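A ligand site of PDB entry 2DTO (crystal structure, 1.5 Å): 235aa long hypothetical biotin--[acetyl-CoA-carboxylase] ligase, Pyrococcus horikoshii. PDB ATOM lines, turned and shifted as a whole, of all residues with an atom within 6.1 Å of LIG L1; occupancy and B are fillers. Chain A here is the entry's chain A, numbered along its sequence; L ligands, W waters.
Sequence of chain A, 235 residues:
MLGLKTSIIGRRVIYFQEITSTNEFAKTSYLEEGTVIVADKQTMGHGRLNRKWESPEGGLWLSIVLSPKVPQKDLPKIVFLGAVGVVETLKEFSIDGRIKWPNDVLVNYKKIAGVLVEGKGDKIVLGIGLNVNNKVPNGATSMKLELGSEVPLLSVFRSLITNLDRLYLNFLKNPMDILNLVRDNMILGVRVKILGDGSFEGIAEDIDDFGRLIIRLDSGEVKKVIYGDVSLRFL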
ATOM      1  N   THR A  20      37.065  14.787  13.158  1.00  0.00           N
ATOM      2  CA  THR A  20      35.855  15.142  12.430  1.00  0.00           C
ATOM      3  C   THR A  20      34.667  14.629  13.253  1.00  0.00           C
ATOM      4  O   THR A  20      33.788  15.383  13.660  1.00  0.00           O
ATOM      5  CB  THR A  20      35.820  14.474  11.043  1.00  0.00           C
ATOM      6  OG1 THR A  20      36.157  13.086  11.169  1.00  0.00           O
ATOM      7  CG2 THR A  20      36.823  15.152  10.106  1.00  0.00           C
ATOM      8  N   SER A  21      34.684  13.323  13.526  1.00  0.00           N
ATOM      9  CA  SER A  21      33.627  12.678  14.294  1.00  0.00           C
ATOM     10  C   SER A  21      34.148  11.350  14.809  1.00  0.00           C
ATOM     11  O   SER A  21      34.661  10.542  14.039  1.00  0.00           O
ATOM     12  CB  SER A  21      32.406  12.430  13.416  1.00  0.00           C
ATOM     13  OG  SER A  21      31.549  11.446  13.973  1.00  0.00           O
ATOM     14  N   THR A  22      34.005  11.109  16.117  1.00  0.00           N
ATOM     15  CA  THR A  22      34.464   9.848  16.678  1.00  0.00           C
ATOM     16  C   THR A  22      33.644   8.676  16.110  1.00  0.00           C
ATOM     17  O   THR A  22      34.174   7.592  15.907  1.00  0.00           O
ATOM     18  CB  THR A  22      34.395   9.855  18.224  1.00  0.00           C
ATOM     19  OG1 THR A  22      33.037  10.070  18.654  1.00  0.00           O
ATOM     20  CG2 THR A  22      35.265  10.957  18.809  1.00  0.00           C
ATOM     21  N   ASN A  23      32.356   8.898  15.849  1.00  0.00           N
ATOM     22  CA  ASN A  23      31.543   7.827  15.295  1.00  0.00           C
ATOM     23  C   ASN A  23      32.015   7.468  13.884  1.00  0.00           C
ATOM     24  O   ASN A  23      32.123   6.286  13.551  1.00  0.00           O
ATOM     25  CB  ASN A  23      30.055   8.222  15.262  1.00  0.00           C
ATOM     26  CG  ASN A  23      29.241   7.517  16.338  1.00  0.00           C
ATOM     27  OD1 ASN A  23      29.692   7.361  17.466  1.00  0.00           O
ATOM     28  ND2 ASN A  23      28.035   7.096  15.981  1.00  0.00           N
ATOM     29  N   GLU A  24      32.326   8.475  13.077  1.00  0.00           N
ATOM     30  CA  GLU A  24      32.796   8.221  11.731  1.00  0.00           C
ATOM     31  C   GLU A  24      34.152   7.510  11.752  1.00  0.00           C
ATOM     32  O   GLU A  24      34.374   6.568  11.001  1.00  0.00           O
ATOM     33  CB  GLU A  24      32.917   9.536  10.934  1.00  0.00           C
ATOM     34  CG  GLU A  24      31.585  10.205  10.663  1.00  0.00           C
ATOM     35  CD  GLU A  24      30.555   9.265  10.045  1.00  0.00           C
ATOM     36  OE1 GLU A  24      30.852   8.647   8.994  1.00  0.00           O
ATOM     37  OE2 GLU A  24      29.448   9.160  10.598  1.00  0.00           O
ATOM     38  N   GLN A  42      35.045  17.971  18.216  1.00  0.00           N
ATOM     39  CA  GLN A  42      34.736  17.403  16.904  1.00  0.00           C
ATOM     40  C   GLN A  42      34.352  18.554  15.986  1.00  0.00           C
ATOM     41  O   GLN A  42      33.659  19.485  16.406  1.00  0.00           O
ATOM     42  CB  GLN A  42      33.549  16.432  16.986  1.00  0.00           C
ATOM     43  CG  GLN A  42      33.722  15.311  17.989  1.00  0.00           C
ATOM     44  CD  GLN A  42      32.572  14.332  17.956  1.00  0.00           C
ATOM     45  OE1 GLN A  42      32.749  13.168  17.606  1.00  0.00           O
ATOM     46  NE2 GLN A  42      31.387  14.792  18.320  1.00  0.00           N
ATOM     47  N   MET A  44      32.932  17.898  12.919  1.00  0.00           N
ATOM     48  CA  MET A  44      31.765  17.432  12.162  1.00  0.00           C
ATOM     49  C   MET A  44      30.960  16.421  12.974  1.00  0.00           C
ATOM     50  O   MET A  44      30.573  15.376  12.456  1.00  0.00           O
ATOM     51  CB  MET A  44      32.221  16.774  10.857  1.00  0.00           C
ATOM     52  CG  MET A  44      33.313  17.529  10.114  1.00  0.00           C
ATOM     53  SD  MET A  44      33.635  16.892   8.312  1.00  0.00           S
ATOM     54  CE  MET A  44      31.907  17.245   7.510  1.00  0.00           C
ATOM     55  N   GLY A  45      30.701  16.743  14.246  1.00  0.00           N
ATOM     56  CA  GLY A  45      29.930  15.842  15.083  1.00  0.00           C
ATOM     57  C   GLY A  45      28.499  15.775  14.595  1.00  0.00           C
ATOM     58  O   GLY A  45      27.964  16.764  14.095  1.00  0.00           O
ATOM     59  N   HIS A  46      27.862  14.623  14.729  1.00  0.00           N
ATOM     60  CA  HIS A  46      26.481  14.508  14.264  1.00  0.00           C
ATOM     61  C   HIS A  46      25.615  13.559  15.068  1.00  0.00           C
ATOM     62  O   HIS A  46      26.119  12.723  15.835  1.00  0.00           O
ATOM     63  CB  HIS A  46      26.476  14.065  12.795  1.00  0.00           C
ATOM     64  CG  HIS A  46      26.963  12.669  12.576  1.00  0.00           C
ATOM     65  ND1 HIS A  46      26.204  11.560  12.846  1.00  0.00           N
ATOM     66  CD2 HIS A  46      28.156  12.208  12.137  1.00  0.00           C
ATOM     67  CE1 HIS A  46      26.903  10.469  12.590  1.00  0.00           C
ATOM     68  NE2 HIS A  46      28.090  10.840  12.160  1.00  0.00           N
ATOM     69  N   GLY A  47      24.308  13.722  14.902  1.00  0.00           N
ATOM     70  CA  GLY A  47      23.343  12.864  15.548  1.00  0.00           C
ATOM     71  C   GLY A  47      22.746  12.080  14.397  1.00  0.00           C
ATOM     72  O   GLY A  47      23.459  11.771  13.438  1.00  0.00           O
ATOM     73  N   ARG A  48      21.456  11.763  14.451  1.00  0.00           N
ATOM     74  CA  ARG A  48      20.831  11.034  13.354  1.00  0.00           C
ATOM     75  C   ARG A  48      20.629  11.960  12.156  1.00  0.00           C
ATOM     76  O   ARG A  48      20.671  13.185  12.301  1.00  0.00           O
ATOM     77  CB  ARG A  48      19.451  10.490  13.755  1.00  0.00           C
ATOM     78  CG  ARG A  48      19.438   9.537  14.927  1.00  0.00           C
ATOM     79  CD  ARG A  48      17.991   9.208  15.270  1.00  0.00           C
ATOM     80  NE  ARG A  48      17.242  10.423  15.611  1.00  0.00           N
ATOM     81  CZ  ARG A  48      15.918  10.495  15.672  1.00  0.00           C
ATOM     82  NH1 ARG A  48      15.174   9.426  15.421  1.00  0.00           N
ATOM     83  NH2 ARG A  48      15.341  11.651  15.994  1.00  0.00           N
ATOM     84  N   TRP A  53      25.908  18.057  15.687  1.00  0.00           N
ATOM     85  CA  TRP A  53      26.063  17.912  17.125  1.00  0.00           C
ATOM     86  C   TRP A  53      27.214  18.816  17.526  1.00  0.00           C
ATOM     87  O   TRP A  53      28.358  18.595  17.133  1.00  0.00           O
ATOM     88  CB  TRP A  53      26.385  16.463  17.506  1.00  0.00           C
ATOM     89  CG  TRP A  53      26.613  16.281  18.987  1.00  0.00           C
ATOM     90  CD1 TRP A  53      27.824  16.307  19.640  1.00  0.00           C
ATOM     91  CD2 TRP A  53      25.617  16.138  19.996  1.00  0.00           C
ATOM     92  NE1 TRP A  53      27.620  16.189  21.004  1.00  0.00           N
ATOM     93  CE2 TRP A  53      26.278  16.090  21.243  1.00  0.00           C
ATOM     94  CE3 TRP A  53      24.214  16.063  19.975  1.00  0.00           C
ATOM     95  CZ2 TRP A  53      25.588  15.953  22.462  1.00  0.00           C
ATOM     96  CZ3 TRP A  53      23.533  15.923  21.176  1.00  0.00           C
ATOM     97  CH2 TRP A  53      24.224  15.874  22.403  1.00  0.00           C
ATOM     98  N   SER A  55      30.151  20.108  19.354  1.00  0.00           N
ATOM     99  CA  SER A  55      31.162  19.407  20.148  1.00  0.00           C
ATOM    100  C   SER A  55      32.366  20.264  20.506  1.00  0.00           C
ATOM    101  O   SER A  55      33.491  19.964  20.110  1.00  0.00           O
ATOM    102  CB  SER A  55      31.637  18.185  19.376  1.00  0.00           C
ATOM    103  OG  SER A  55      30.549  17.483  18.800  1.00  0.00           O
ATOM    104  N   LEU A  60      32.448  15.675  26.695  1.00  0.00           N
ATOM    105  CA  LEU A  60      32.953  14.308  26.523  1.00  0.00           C
ATOM    106  C   LEU A  60      32.323  13.747  25.250  1.00  0.00           C
ATOM    107  O   LEU A  60      31.123  13.447  25.207  1.00  0.00           O
ATOM    108  CB  LEU A  60      32.578  13.452  27.739  1.00  0.00           C
ATOM    109  CG  LEU A  60      33.204  12.060  27.788  1.00  0.00           C
ATOM    110  CD1 LEU A  60      34.724  12.165  27.801  1.00  0.00           C
ATOM    111  CD2 LEU A  60      32.713  11.320  29.036  1.00  0.00           C
ATOM    112  N   TRP A  61      33.148  13.614  24.212  1.00  0.00           N
ATOM    113  CA  TRP A  61      32.697  13.122  22.917  1.00  0.00           C
ATOM    114  C   TRP A  61      33.428  11.816  22.635  1.00  0.00           C
ATOM    115  O   TRP A  61      34.640  11.801  22.418  1.00  0.00           O
ATOM    116  CB  TRP A  61      33.039  14.164  21.835  1.00  0.00           C
ATOM    117  CG  TRP A  61      32.902  15.612  22.286  1.00  0.00           C
ATOM    118  CD1 TRP A  61      33.884  16.569  22.280  1.00  0.00           C
ATOM    119  CD2 TRP A  61      31.735  16.250  22.833  1.00  0.00           C
ATOM    120  NE1 TRP A  61      33.407  17.756  22.776  1.00  0.00           N
ATOM    121  CE2 TRP A  61      32.089  17.589  23.121  1.00  0.00           C
ATOM    122  CE3 TRP A  61      30.431  15.816  23.098  1.00  0.00           C
ATOM    123  CZ2 TRP A  61      31.183  18.500  23.671  1.00  0.00           C
ATOM    124  CZ3 TRP A  61      29.523  16.736  23.645  1.00  0.00           C
ATOM    125  CH2 TRP A  61      29.911  18.056  23.920  1.00  0.00           C
ATOM    126  N   LEU A  62      32.707  10.704  22.641  1.00  0.00           N
ATOM    127  CA  LEU A  62      33.352   9.430  22.412  1.00  0.00           C
ATOM    128  C   LEU A  62      32.495   8.392  21.717  1.00  0.00           C
ATOM    129  O   LEU A  62      31.267   8.504  21.645  1.00  0.00           O
ATOM    130  CB  LEU A  62      33.875   8.860  23.736  1.00  0.00           C
ATOM    131  CG  LEU A  62      32.863   8.557  24.853  1.00  0.00           C
ATOM    132  CD1 LEU A  62      32.112   7.263  24.571  1.00  0.00           C
ATOM    133  CD2 LEU A  62      33.605   8.441  26.176  1.00  0.00           C
ATOM    134  N   SER A  63      33.171   7.386  21.170  1.00  0.00           N
ATOM    135  CA  SER A  63      32.506   6.275  20.503  1.00  0.00           C
ATOM    136  C   SER A  63      33.195   4.999  20.950  1.00  0.00           C
ATOM    137  O   SER A  63      34.395   4.985  21.212  1.00  0.00           O
ATOM    138  CB  SER A  63      32.639   6.417  18.987  1.00  0.00           C
ATOM    139  OG  SER A  63      32.011   7.599  18.546  1.00  0.00           O
ATOM    140  N   ASN A 103      17.220   7.545  23.368  1.00  0.00           N
ATOM    141  CA  ASN A 103      18.613   7.970  23.225  1.00  0.00           C
ATOM    142  C   ASN A 103      19.088   9.251  23.900  1.00  0.00           C
ATOM    143  O   ASN A 103      20.257   9.621  23.743  1.00  0.00           O
ATOM    144  CB  ASN A 103      18.897   8.096  21.738  1.00  0.00           C
ATOM    145  CG  ASN A 103      18.090   9.213  21.093  1.00  0.00           C
ATOM    146  OD1 ASN A 103      17.034   9.597  21.614  1.00  0.00           O
ATOM    147  ND2 ASN A 103      18.572   9.738  19.980  1.00  0.00           N
ATOM    148  N   ASP A 104      18.216   9.928  24.632  1.00  0.00           N
ATOM    149  CA  ASP A 104      18.607  11.180  25.263  1.00  0.00           C
ATOM    150  C   ASP A 104      18.558  11.160  26.779  1.00  0.00           C
ATOM    151  O   ASP A 104      17.800  10.402  27.386  1.00  0.00           O
ATOM    152  CB  ASP A 104      17.702  12.322  24.757  1.00  0.00           C
ATOM    153  CG  ASP A 104      17.778  12.522  23.257  1.00  0.00           C
ATOM    154  OD1 ASP A 104      18.874  12.428  22.688  1.00  0.00           O
ATOM    155  OD2 ASP A 104      16.725  12.804  22.642  1.00  0.00           O
ATOM    156  N   LYS A 111      18.391  18.837  27.616  1.00  0.00           N
ATOM    157  CA  LYS A 111      19.282  17.792  27.123  1.00  0.00           C
ATOM    158  C   LYS A 111      20.740  17.971  27.542  1.00  0.00           C
ATOM    159  O   LYS A 111      21.376  18.983  27.236  1.00  0.00           O
ATOM    160  CB  LYS A 111      19.161  17.707  25.608  1.00  0.00           C
ATOM    161  CG  LYS A 111      19.920  16.541  24.979  1.00  0.00           C
ATOM    162  CD  LYS A 111      19.502  16.389  23.531  1.00  0.00           C
ATOM    163  CE  LYS A 111      20.240  15.247  22.853  1.00  0.00           C
ATOM    164  NZ  LYS A 111      19.809  15.134  21.435  1.00  0.00           N
ATOM    165  N   ALA A 113      22.870  15.056  27.314  1.00  0.00           N
ATOM    166  CA  ALA A 113      23.608  14.039  26.562  1.00  0.00           C
ATOM    167  C   ALA A 113      22.766  13.356  25.499  1.00  0.00           C
ATOM    168  O   ALA A 113      21.539  13.286  25.594  1.00  0.00           O
ATOM    169  CB  ALA A 113      24.163  12.991  27.537  1.00  0.00           C
ATOM    170  N   GLY A 114      23.442  12.849  24.478  1.00  0.00           N
ATOM    171  CA  GLY A 114      22.767  12.158  23.393  1.00  0.00           C
ATOM    172  C   GLY A 114      23.572  10.937  23.002  1.00  0.00           C
ATOM    173  O   GLY A 114      24.810  10.961  23.025  1.00  0.00           O
ATOM    174  N   VAL A 115      22.862   9.879  22.629  1.00  0.00           N
ATOM    175  CA  VAL A 115      23.470   8.610  22.234  1.00  0.00           C
ATOM    176  C   VAL A 115      23.104   8.329  20.784  1.00  0.00           C
ATOM    177  O   VAL A 115      21.970   8.559  20.357  1.00  0.00           O
ATOM    178  CB  VAL A 115      22.938   7.459  23.117  1.00  0.00           C
ATOM    179  CG1 VAL A 115      23.623   6.151  22.756  1.00  0.00           C
ATOM    180  CG2 VAL A 115      23.165   7.796  24.590  1.00  0.00           C
ATOM    181  N   LEU A 116      24.079   7.823  20.027  1.00  0.00           N
ATOM    182  CA  LEU A 116      23.868   7.481  18.629  1.00  0.00           C
ATOM    183  C   LEU A 116      24.558   6.168  18.317  1.00  0.00           C
ATOM    184  O   LEU A 116      25.782   6.082  18.405  1.00  0.00           O
ATOM    185  CB  LEU A 116      24.439   8.561  17.703  1.00  0.00           C
ATOM    186  CG  LEU A 116      24.329   8.247  16.200  1.00  0.00           C
ATOM    187  CD1 LEU A 116      22.866   8.186  15.786  1.00  0.00           C
ATOM    188  CD2 LEU A 116      25.058   9.310  15.396  1.00  0.00           C
ATOM    189  N   GLY A 127      27.968   5.680  20.065  1.00  0.00           N
ATOM    190  CA  GLY A 127      28.464   7.039  20.235  1.00  0.00           C
ATOM    191  C   GLY A 127      27.741   7.766  21.342  1.00  0.00           C
ATOM    192  O   GLY A 127      26.525   7.631  21.490  1.00  0.00           O
ATOM    193  N   ILE A 128      28.488   8.536  22.126  1.00  0.00           N
ATOM    194  CA  ILE A 128      27.927   9.274  23.240  1.00  0.00           C
ATOM    195  C   ILE A 128      28.510  10.676  23.327  1.00  0.00           C
ATOM    196  O   ILE A 128      29.729  10.853  23.307  1.00  0.00           O
ATOM    197  CB  ILE A 128      28.223   8.549  24.582  1.00  0.00           C
ATOM    198  CG1 ILE A 128      27.628   7.136  24.536  1.00  0.00           C
ATOM    199  CG2 ILE A 128      27.648   9.349  25.765  1.00  0.00           C
ATOM    200  CD1 ILE A 128      27.993   6.277  25.751  1.00  0.00           C
ATOM    201  N   GLY A 129      27.626  11.670  23.418  1.00  0.00           N
ATOM    202  CA  GLY A 129      28.048  13.050  23.560  1.00  0.00           C
ATOM    203  C   GLY A 129      27.446  13.540  24.857  1.00  0.00           C
ATOM    204  O   GLY A 129      26.235  13.499  25.031  1.00  0.00           O
ATOM    205  N   LEU A 130      28.296  13.971  25.790  1.00  0.00           N
ATOM    206  CA  LEU A 130      27.840  14.457  27.089  1.00  0.00           C
ATOM    207  C   LEU A 130      28.423  15.833  27.364  1.00  0.00           C
ATOM    208  O   LEU A 130      29.640  16.003  27.355  1.00  0.00           O
ATOM    209  CB  LEU A 130      28.266  13.478  28.190  1.00  0.00           C
ATOM    210  CG  LEU A 130      28.131  13.914  29.652  1.00  0.00           C
ATOM    211  CD1 LEU A 130      26.665  14.089  30.017  1.00  0.00           C
ATOM    212  CD2 LEU A 130      28.789  12.858  30.541  1.00  0.00           C
HETATM  213  C1  LIG L   1      21.667  12.322  20.007  1.00  0.00           C
HETATM  214  O1  LIG L   1      20.859  11.492  20.517  1.00  0.00           O
HETATM  215  O2  LIG L   1      21.468  13.572  20.068  1.00  0.00           O
HETATM  216  C2  LIG L   1      22.926  11.884  19.300  1.00  0.00           C
HETATM  217  C3  LIG L   1      24.216  12.583  19.509  1.00  0.00           C
HETATM  218  C4  LIG L   1      25.419  11.709  19.507  1.00  0.00           C
HETATM  219  C5  LIG L   1      26.672  12.518  19.752  1.00  0.00           C
HETATM  220  C6  LIG L   1      27.997  11.758  19.804  1.00  0.00           C
HETATM  221  S1  LIG L   1      29.391  12.827  20.112  1.00  0.00           S
HETATM  222  C7  LIG L   1      30.430  11.348  19.980  1.00  0.00           C
HETATM  223  C8  LIG L   1      29.911  10.725  18.649  1.00  0.00           C
HETATM  224  N1  LIG L   1      30.519  11.352  17.448  1.00  0.00           N
HETATM  225  C9  LIG L   1      29.528  11.902  16.665  1.00  0.00           C
HETATM  226  O3  LIG L   1      29.700  12.510  15.591  1.00  0.00           O
HETATM  227  N2  LIG L   1      28.285  11.695  17.246  1.00  0.00           N
HETATM  228  C10 LIG L   1      28.398  10.960  18.493  1.00  0.00           C
HETATM  229  P1  LG2 L   2      15.542  15.511  18.183  1.00  0.00           P
HETATM  230  O1  LG2 L   2      16.381  16.751  18.315  1.00  0.00           O
HETATM  231  O2  LG2 L   2      14.628  15.649  16.966  1.00  0.00           O
HETATM  232  O3  LG2 L   2      14.704  15.328  19.445  1.00  0.00           O
HETATM  233  P2  LG2 L   2      17.420  13.356  18.893  1.00  0.00           P
HETATM  234  O4  LG2 L   2      17.122  11.889  18.874  1.00  0.00           O
HETATM  235  O5  LG2 L   2      17.273  13.885  20.282  1.00  0.00           O
HETATM  236  O6  LG2 L   2      16.438  14.176  17.849  1.00  0.00           O
HETATM  237  P3  LG2 L   2      19.449  13.530  16.872  1.00  0.00           P
HETATM  238  O7  LG2 L   2      20.199  12.273  16.700  1.00  0.00           O
HETATM  239  O8  LG2 L   2      18.320  13.569  15.904  1.00  0.00           O
HETATM  240  O9  LG2 L   2      18.904  13.720  18.400  1.00  0.00           O
HETATM  241  O10 LG2 L   2      20.525  14.705  16.657  1.00  0.00           O
HETATM  242  C1  LG2 L   2      20.932  15.680  17.686  1.00  0.00           C
HETATM  243  C2  LG2 L   2      20.135  16.943  17.970  1.00  0.00           C
HETATM  244  O11 LG2 L   2      20.642  17.427  19.271  1.00  0.00           O
HETATM  245  C3  LG2 L   2      20.330  18.115  17.015  1.00  0.00           C
HETATM  246  O12 LG2 L   2      19.303  18.129  16.010  1.00  0.00           O
HETATM  247  C4  LG2 L   2      20.370  19.321  17.942  1.00  0.00           C
HETATM  248  O13 LG2 L   2      19.103  19.990  18.040  1.00  0.00           O
HETATM  249  C5  LG2 L   2      20.778  18.840  19.316  1.00  0.00           C
HETATM  250  N1  LG2 L   2      22.181  19.107  19.778  1.00  0.00           N
HETATM  251  C6  LG2 L   2      23.351  19.380  19.046  1.00  0.00           C
HETATM  252  N2  LG2 L   2      24.429  19.570  19.791  1.00  0.00           N
HETATM  253  C7  LG2 L   2      23.977  19.405  21.084  1.00  0.00           C
HETATM  254  C8  LG2 L   2      24.633  19.465  22.371  1.00  0.00           C
HETATM  255  N3  LG2 L   2      25.948  19.724  22.523  1.00  0.00           N
HETATM  256  N4  LG2 L   2      23.856  19.251  23.533  1.00  0.00           N
HETATM  257  C9  LG2 L   2      22.510  18.992  23.400  1.00  0.00           C
HETATM  258  N5  LG2 L   2      21.799  18.909  22.239  1.00  0.00           N
HETATM  259  C10 LG2 L   2      22.588  19.123  21.105  1.00  0.00           C
HETATM  260  O   HOH W   1      20.503   9.643  17.907  1.00  0.00           O
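Water W1 lies within hydrogen-bond range of ND2 of Asn 103 (2.8 Å), O7 of LG2 L2 (2.9 Å), O of Val 115 (3.1 Å) and O1 of LIG L1 (3.2 Å).
The backbone NH (N) of Asn 23 lies close to a nitrogen (N1) of LIG L1, 3.5 Å away. A sulfur (S1) of LIG L1 lies close to the backbone carbonyl oxygen (O) of Ile 128, at 3.8 Å. Gly 45 touches LIG L1 (CA to O3, 3.4 Å). Gly 47 touches LIG L1. CZ3 of Trp 53 touches O2 of LIG L1, at 3.3 Å. Leu 62 touches LIG L1. Ser 63 touches LIG L1. CA of Gly 114 touches O1 of LIG L1, 3.5 Å away. Leu 116 touches LIG L1. N of Gly 129 touches C6 of LIG L1, at 3.6 Å. Hydrophobic or aromatic side chains within 4 Å of LIG L1: His 46, Trp 53 and Leu 116.
An oxygen (O9) of LG2 L2 sits close to an oxygen (O2) of LIG L1, 3.1 Å away.
The backbone NH of Arg 48 is in hydrogen-bond range of an oxygen (O7) of LG2 L2 (2.6 Å). NZ of Lys 111 lies within salt-bridge range of O5 of LG2 L2, 3.1 Å away. An oxygen (O1) of LIG L1 lies within hydrogen-bond range of the backbone NH (N) of Val 115 (3.3 Å). The backbone carbonyl oxygen of His 46 sits at hydrogen-bond distance from a nitrogen (N2) of LIG L1 (2.8 Å). O3 of LIG L1 is in hydrogen-bond range of OG of Ser 21 (2.7 Å). N1 of LIG L1 is in hydrogen-bond range of OG1 of Thr 22, at 3.1 Å. O1 of LIG L1 is in hydrogen-bond range of ND2 of Asn 103 (2.9 Å). The side-chain amide oxygen (OE1) of Gln 42 is in hydrogen-bond range of a nitrogen (N1) of LIG L1, 2.9 Å away. O8 of LG2 L2 lies within salt-bridge range of NE of Arg 48, at 3.3 Å. An oxygen (O2) of LIG L1 lies within salt-bridge range of the side-chain amino group (NZ) of Lys 111 (2.7 Å). The side-chain carboxylate (OD2) of Asp 104 sits close to an oxygen (O5) of LG2 L2, 2.7 Å away. The backbone NH of His 46 sits at hydrogen-bond distance from an oxygen (O3) of LIG L1 (2.9 Å). The side-chain amide nitrogen (ND2) of Asn 103 is in hydrogen-bond range of an oxygen (O4) of LG2 L2, at 2.8 Å. OD1 of Asp 104 lies close to O1 of LIG L1 (3.1 Å).
The side-chain amide oxygen (OE1) of Gln 42 sits at hydrogen-bond distance from the backbone NH (N) of Thr 22. The side-chain amide oxygen (OD1) of Asn 23 sits at hydrogen-bond distance from the side-chain hydroxyl (OG) of Ser 63, 2.6 Å away. OD2 of Asp 104 lies close to OD1 of Asn 103, 3.4 Å away. The backbone carbonyl oxygen of Trp 53 sits at hydrogen-bond distance from the side-chain hydroxyl of Ser 55. The side-chain hydroxyl (OG1) of Thr 22 lies within hydrogen-bond range of the side-chain hydroxyl (OG) of Ser 63, at 2.7 Å. The backbone NH of Val 115 sits at hydrogen-bond distance from the backbone carbonyl oxygen of Asn 103 (2.8 Å). O of Leu 116 sits at hydrogen-bond distance from ND2 of Asn 23. N of Trp 53 sits at hydrogen-bond distance from O of Gly 45 (2.9 Å).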
